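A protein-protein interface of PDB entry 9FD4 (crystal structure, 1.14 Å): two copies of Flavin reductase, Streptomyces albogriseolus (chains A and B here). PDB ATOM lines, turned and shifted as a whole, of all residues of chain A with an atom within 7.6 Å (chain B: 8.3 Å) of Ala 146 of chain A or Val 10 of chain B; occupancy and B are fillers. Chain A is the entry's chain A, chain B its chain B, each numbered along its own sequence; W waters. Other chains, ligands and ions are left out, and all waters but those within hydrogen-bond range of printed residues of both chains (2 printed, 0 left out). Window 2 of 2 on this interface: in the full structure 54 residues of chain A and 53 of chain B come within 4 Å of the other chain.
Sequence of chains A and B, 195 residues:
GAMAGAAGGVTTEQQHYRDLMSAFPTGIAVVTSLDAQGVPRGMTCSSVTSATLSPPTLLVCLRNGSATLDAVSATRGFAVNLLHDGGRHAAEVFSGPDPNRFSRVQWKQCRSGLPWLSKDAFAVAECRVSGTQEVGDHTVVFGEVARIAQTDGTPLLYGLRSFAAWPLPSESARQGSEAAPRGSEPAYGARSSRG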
ATOM      1  N   PRO A  56     -14.529  -0.970  33.585  1.00  0.00           N
ATOM      2  CA  PRO A  56     -13.960  -2.198  34.168  1.00  0.00           C
ATOM      3  C   PRO A  56     -12.867  -2.759  33.275  1.00  0.00           C
ATOM      4  O   PRO A  56     -13.108  -3.098  32.113  1.00  0.00           O
ATOM      5  CB  PRO A  56     -15.182  -3.122  34.270  1.00  0.00           C
ATOM      6  CG  PRO A  56     -16.336  -2.153  34.509  1.00  0.00           C
ATOM      7  CD  PRO A  56     -16.010  -0.992  33.598  1.00  0.00           C
ATOM      8  N   PHE A  78     -10.493 -11.350  23.895  1.00  0.00           N
ATOM      9  CA  PHE A  78     -10.185 -12.579  24.604  1.00  0.00           C
ATOM     10  C   PHE A  78     -11.240 -12.804  25.666  1.00  0.00           C
ATOM     11  O   PHE A  78     -11.885 -11.870  26.120  1.00  0.00           O
ATOM     12  CB  PHE A  78      -8.767 -12.555  25.207  1.00  0.00           C
ATOM     13  CG  PHE A  78      -8.512 -11.495  26.269  1.00  0.00           C
ATOM     14  CD1 PHE A  78      -8.155 -10.202  25.915  1.00  0.00           C
ATOM     15  CD2 PHE A  78      -8.578 -11.786  27.605  1.00  0.00           C
ATOM     16  CE1 PHE A  78      -7.817  -9.269  26.881  1.00  0.00           C
ATOM     17  CE2 PHE A  78      -8.278 -10.856  28.571  1.00  0.00           C
ATOM     18  CZ  PHE A  78      -7.896  -9.587  28.217  1.00  0.00           C
ATOM     19  N   ALA A 125     -15.627 -13.946  31.204  1.00  0.00           N
ATOM     20  CA  ALA A 125     -15.597 -12.519  30.942  1.00  0.00           C
ATOM     21  C   ALA A 125     -15.021 -12.275  29.556  1.00  0.00           C
ATOM     22  O   ALA A 125     -13.864 -12.625  29.295  1.00  0.00           O
ATOM     23  CB  ALA A 125     -14.773 -11.770  31.976  1.00  0.00           C
ATOM     24  N   GLU A 126     -15.814 -11.656  28.691  1.00  0.00           N
ATOM     25  CA  GLU A 126     -15.353 -11.286  27.355  1.00  0.00           C
ATOM     26  C   GLU A 126     -14.754  -9.893  27.400  1.00  0.00           C
ATOM     27  O   GLU A 126     -15.387  -8.975  27.911  1.00  0.00           O
ATOM     28  CB  GLU A 126     -16.488 -11.310  26.337  1.00  0.00           C
ATOM     29  CG  GLU A 126     -17.164 -12.626  26.180  1.00  0.00           C
ATOM     30  CD  GLU A 126     -18.020 -12.685  24.950  1.00  0.00           C
ATOM     31  OE1 GLU A 126     -17.552 -12.214  23.890  1.00  0.00           O
ATOM     32  OE2 GLU A 126     -19.101 -13.284  25.008  1.00  0.00           O
ATOM     33  N   CYS A 127     -13.550  -9.752  26.850  1.00  0.00           N
ATOM     34  CA  CYS A 127     -12.752  -8.544  26.966  1.00  0.00           C
ATOM     35  C   CYS A 127     -12.296  -8.054  25.602  1.00  0.00           C
ATOM     36  O   CYS A 127     -11.961  -8.846  24.715  1.00  0.00           O
ATOM     37  CB  CYS A 127     -11.517  -8.822  27.806  1.00  0.00           C
ATOM     38  SG  CYS A 127     -11.875  -9.427  29.493  1.00  0.00           S
ATOM     39  N   ARG A 128     -12.251  -6.738  25.460  1.00  0.00           N
ATOM     40  CA  ARG A 128     -11.591  -6.084  24.339  1.00  0.00           C
ATOM     41  C   ARG A 128     -10.212  -5.643  24.780  1.00  0.00           C
ATOM     42  O   ARG A 128     -10.056  -5.068  25.866  1.00  0.00           O
ATOM     43  CB  ARG A 128     -12.349  -4.825  23.894  1.00  0.00           C
ATOM     44  CG  ARG A 128     -13.645  -5.022  23.188  1.00  0.00           C
ATOM     45  CD  ARG A 128     -14.205  -3.664  22.736  1.00  0.00           C
ATOM     46  NE  ARG A 128     -14.537  -2.811  23.875  1.00  0.00           N
ATOM     47  CZ  ARG A 128     -15.673  -2.904  24.563  1.00  0.00           C
ATOM     48  NH1 ARG A 128     -16.641  -3.724  24.185  1.00  0.00           N
ATOM     49  NH2 ARG A 128     -15.854  -2.128  25.631  1.00  0.00           N
ATOM     50  N   GLY A 143      -7.526  -5.589  29.315  1.00  0.00           N
ATOM     51  CA  GLY A 143      -8.812  -5.987  28.788  1.00  0.00           C
ATOM     52  C   GLY A 143      -9.947  -5.216  29.411  1.00  0.00           C
ATOM     53  O   GLY A 143     -10.218  -5.347  30.609  1.00  0.00           O
ATOM     54  N   GLU A 144     -10.641  -4.449  28.588  1.00  0.00           N
ATOM     55  CA  GLU A 144     -11.866  -3.793  29.007  1.00  0.00           C
ATOM     56  C   GLU A 144     -12.991  -4.801  28.903  1.00  0.00           C
ATOM     57  O   GLU A 144     -13.193  -5.411  27.852  1.00  0.00           O
ATOM     58  CB  GLU A 144     -12.160  -2.538  28.182  1.00  0.00           C
ATOM     59  CG  GLU A 144     -11.206  -1.413  28.596  1.00  0.00           C
ATOM     60  CD  GLU A 144     -11.382  -0.110  27.857  1.00  0.00           C
ATOM     61  OE1 GLU A 144     -12.165  -0.057  26.909  1.00  0.00           O
ATOM     62  OE2 GLU A 144     -10.660   0.849  28.218  1.00  0.00           O
ATOM     63  N   VAL A 145     -13.679  -5.029  30.013  1.00  0.00           N
ATOM     64  CA  VAL A 145     -14.646  -6.110  30.093  1.00  0.00           C
ATOM     65  C   VAL A 145     -15.978  -5.691  29.476  1.00  0.00           C
ATOM     66  O   VAL A 145     -16.617  -4.729  29.925  1.00  0.00           O
ATOM     67  CB  VAL A 145     -14.813  -6.583  31.536  1.00  0.00           C
ATOM     68  CG1 VAL A 145     -15.779  -7.783  31.568  1.00  0.00           C
ATOM     69  CG2 VAL A 145     -13.471  -7.014  32.168  1.00  0.00           C
ATOM     70  N   ALA A 146     -16.381  -6.417  28.442  1.00  0.00           N
ATOM     71  CA  ALA A 146     -17.589  -6.177  27.670  1.00  0.00           C
ATOM     72  C   ALA A 146     -18.785  -6.932  28.226  1.00  0.00           C
ATOM     73  O   ALA A 146     -19.896  -6.411  28.184  1.00  0.00           O
ATOM     74  CB  ALA A 146     -17.370  -6.585  26.208  1.00  0.00           C
ATOM     75  N   ARG A 147     -18.586  -8.154  28.707  1.00  0.00           N
ATOM     76  CA  ARG A 147     -19.689  -9.021  29.111  1.00  0.00           C
ATOM     77  C   ARG A 147     -19.165 -10.010  30.132  1.00  0.00           C
ATOM     78  O   ARG A 147     -18.077 -10.550  29.948  1.00  0.00           O
ATOM     79  CB  ARG A 147     -20.260  -9.788  27.903  1.00  0.00           C
ATOM     80  CG  ARG A 147     -21.500 -10.561  28.250  1.00  0.00           C
ATOM     81  CD  ARG A 147     -22.032 -11.375  27.100  1.00  0.00           C
ATOM     82  NE  ARG A 147     -21.191 -12.533  26.813  1.00  0.00           N
ATOM     83  CZ  ARG A 147     -21.316 -13.720  27.385  1.00  0.00           C
ATOM     84  NH1 ARG A 147     -22.210 -13.947  28.315  1.00  0.00           N
ATOM     85  NH2 ARG A 147     -20.529 -14.707  26.994  1.00  0.00           N
ATOM     86  N   ILE A 148     -19.961 -10.279  31.166  1.00  0.00           N
ATOM     87  CA  ILE A 148     -19.674 -11.307  32.152  1.00  0.00           C
ATOM     88  C   ILE A 148     -20.879 -12.216  32.267  1.00  0.00           C
ATOM     89  O   ILE A 148     -22.021 -11.740  32.286  1.00  0.00           O
ATOM     90  CB  ILE A 148     -19.342 -10.689  33.522  1.00  0.00           C
ATOM     91  CG1 ILE A 148     -18.095  -9.817  33.413  1.00  0.00           C
ATOM     92  CG2 ILE A 148     -19.152 -11.792  34.558  1.00  0.00           C
ATOM     93  CD1 ILE A 148     -17.896  -8.898  34.594  1.00  0.00           C
ATOM     94  N   GLY B   9     -18.623  -1.709  21.701  1.00  0.00           N
ATOM     95  CA  GLY B   9     -18.689  -0.636  22.677  1.00  0.00           C
ATOM     96  C   GLY B   9     -19.343  -1.091  23.968  1.00  0.00           C
ATOM     97  O   GLY B   9     -19.308  -0.368  24.964  1.00  0.00           O
ATOM     98  N   VAL B  10     -19.935  -2.293  23.960  1.00  0.00           N
ATOM     99  CA  VAL B  10     -20.657  -2.782  25.131  1.00  0.00           C
ATOM    100  C   VAL B  10     -19.691  -2.920  26.302  1.00  0.00           C
ATOM    101  O   VAL B  10     -18.544  -3.333  26.141  1.00  0.00           O
ATOM    102  CB  VAL B  10     -21.337  -4.100  24.722  1.00  0.00           C
ATOM    103  CG1 VAL B  10     -21.718  -4.950  25.888  1.00  0.00           C
ATOM    104  CG2 VAL B  10     -22.551  -3.812  23.827  1.00  0.00           C
ATOM    105  N   THR B  11     -20.148  -2.553  27.493  1.00  0.00           N
ATOM    106  CA  THR B  11     -19.320  -2.484  28.687  1.00  0.00           C
ATOM    107  C   THR B  11     -20.104  -3.054  29.849  1.00  0.00           C
ATOM    108  O   THR B  11     -21.253  -2.665  30.062  1.00  0.00           O
ATOM    109  CB  THR B  11     -18.969  -1.017  28.981  1.00  0.00           C
ATOM    110  OG1 THR B  11     -18.226  -0.469  27.877  1.00  0.00           O
ATOM    111  CG2 THR B  11     -18.162  -0.855  30.274  1.00  0.00           C
ATOM    112  N   THR B  12     -19.487  -3.955  30.611  1.00  0.00           N
ATOM    113  CA  THR B  12     -20.169  -4.540  31.758  1.00  0.00           C
ATOM    114  C   THR B  12     -20.337  -3.507  32.871  1.00  0.00           C
ATOM    115  O   THR B  12     -19.602  -2.522  32.965  1.00  0.00           O
ATOM    116  CB  THR B  12     -19.425  -5.773  32.275  1.00  0.00           C
ATOM    117  OG1 THR B  12     -20.255  -6.505  33.172  1.00  0.00           O
ATOM    118  CG2 THR B  12     -18.158  -5.368  32.989  1.00  0.00           C
ATOM    119  N   GLU B  13     -21.301  -3.763  33.741  1.00  0.00           N
ATOM    120  CA  GLU B  13     -21.501  -2.904  34.896  1.00  0.00           C
ATOM    121  C   GLU B  13     -20.424  -3.150  35.948  1.00  0.00           C
ATOM    122  O   GLU B  13     -19.922  -4.262  36.114  1.00  0.00           O
ATOM    123  CB  GLU B  13     -22.872  -3.169  35.522  1.00  0.00           C
ATOM    124  CG  GLU B  13     -24.092  -3.090  34.585  1.00  0.00           C
ATOM    125  CD  GLU B  13     -24.366  -1.706  34.020  1.00  0.00           C
ATOM    126  OE1 GLU B  13     -23.975  -0.699  34.639  1.00  0.00           O
ATOM    127  OE2 GLU B  13     -25.007  -1.633  32.945  1.00  0.00           O
ATOM    128  N   TYR B  17     -18.481  -6.679  37.442  1.00  0.00           N
ATOM    129  CA  TYR B  17     -17.036  -6.828  37.435  1.00  0.00           C
ATOM    130  C   TYR B  17     -16.486  -7.117  38.827  1.00  0.00           C
ATOM    131  O   TYR B  17     -15.633  -7.985  38.990  1.00  0.00           O
ATOM    132  CB  TYR B  17     -16.411  -5.587  36.813  1.00  0.00           C
ATOM    133  CG  TYR B  17     -14.897  -5.579  36.822  1.00  0.00           C
ATOM    134  CD1 TYR B  17     -14.179  -6.315  35.908  1.00  0.00           C
ATOM    135  CD2 TYR B  17     -14.212  -4.894  37.787  1.00  0.00           C
ATOM    136  CE1 TYR B  17     -12.821  -6.339  35.933  1.00  0.00           C
ATOM    137  CE2 TYR B  17     -12.825  -4.894  37.820  1.00  0.00           C
ATOM    138  CZ  TYR B  17     -12.144  -5.628  36.868  1.00  0.00           C
ATOM    139  OH  TYR B  17     -10.787  -5.691  36.884  1.00  0.00           O
HETATM  140  O   HOH W   1     -22.009  -8.286  31.888  1.00  0.00           O
HETATM  141  O   HOH W   2     -15.310  -0.502  28.183  1.00  0.00           O
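The guanidinium group (NH1) of Arg 128 of chain A is in hydrogen-bond range of the backbone carbonyl oxygen (O) of Val 10 of chain B. The backbone carbonyl oxygen (O) of Val 145 of chain A sits at hydrogen-bond distance from the backbone NH (N) of Thr 12 of chain B, 3.1 Å away. The backbone NH (N) of Thr 12 of chain B sits at hydrogen-bond distance from the backbone carbonyl oxygen (O) of Ala 146 of chain A.
N of Val 145 of chain A lies within hydrogen-bond range of O of Pro 56 of chain A (2.9 Å). O of Glu 126 of chain A sits at hydrogen-bond distance from N of Ala 146 of chain A (2.8 Å). The backbone carbonyl oxygen of Arg 128 of chain A sits at hydrogen-bond distance from the backbone NH of Glu 144 of chain A, at 2.9 Å. O of Gly 9 of chain B lies within hydrogen-bond range of OG1 of Thr 11 of chain B (3.1 Å).
Among the printed residues, merely in contact across the chains: Pro 56 of chain A with Thr 11 of chain B (3.96 Å), Pro 56 of chain A with Thr 12 of chain B (3.6 Å), Pro 56 of chain A with Tyr 17 of chain B (3.6 Å), Arg 128 of chain A with Gly 9 of chain B (3.8 Å), Arg 128 of chain A with Thr 11 of chain B (3.7 Å), Val 145 of chain A with Thr 11 of chain B (3.7 Å), Val 145 of chain A with Tyr 17 of chain B (3.9 Å), Ala 146 of chain A with Val 10 of chain B (3.3 Å), Ala 146 of chain A with Thr 11 of chain B (3.8 Å), Ile 148 of chain A with Thr 12 of chain B (3.6 Å) and Ile 148 of chain A with Tyr 17 of chain B (3.6 Å).
Printed residues of chain B within 4 Å of Pro 56 of chain A: Thr 11, Thr 12 and Tyr 17. Cys 127 of chain A touches none of the printed residues of chain B. Of the printed residues of chain B, Arg 128 of chain A touches Gly 9 (3.8 Å), Val 10 (2.8 Å) and Thr 11 (3.7 Å). Of chain B, only Val 10 (3.3 Å), Thr 11 (3.8 Å) and Thr 12 (3.5 Å) come within 4 Å of Ala 146 of chain A. Of the printed residues of chain B, Ile 148 of chain A touches Thr 12 and Tyr 17. Of the printed residues of chain A, Gly 9 of chain B touches Arg 128 (3.8 Å). Val 10 of chain B touches just these residues of chain A: Arg 128 and Ala 146. Of the printed residues of chain A, Thr 12 of chain B touches Pro 56, Val 145, Ala 146 and Ile 148. Glu 13 of chain B touches none of the printed residues of chain A. The nearest residue of chain B that does not touch Ala 146 of chain A is Gly 9 of chain B (6.3 Å). The nearest residue of chain A that does not touch Val 10 of chain B is Val 145 of chain A (4.5 Å).
Of the 6 printed residues of chain B, 5 touch a printed residue of chain A. Printed residues of chain B that touch a printed residue of chain A: Gly 9, Val 10, Thr 11, Thr 12 and Tyr 17. Hydrophobic or aromatic side chains of chain B within 4 Å of the printed part of chain A: Val 10 and Tyr 17. Hydrophobic or aromatic side chains of chain A that line the printed part of chain B: Pro 56, Val 145, Ala 146 and Ile 148. Along chain A the printed residues that touch a printed residue of chain B span positions 56 to 148. Among the printed residues, no Asp or Glu carboxylate lies within 4 Å of a Lys or Arg side-chain nitrogen of the other chain.
No position is printed for both chains.
Water W1 lies within hydrogen-bond range of the side-chain hydroxyl of Thr 12 of chain B (2.8 Å) and the backbone NH of Ile 148 of chain A (2.9 Å). Water W2 lies within hydrogen-bond range of OG1 of Thr 11 of chain B (2.9 Å), NH2 of Arg 128 of chain A (3.1 Å) and OE1 of Glu 144 of chain A (3.4 Å).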
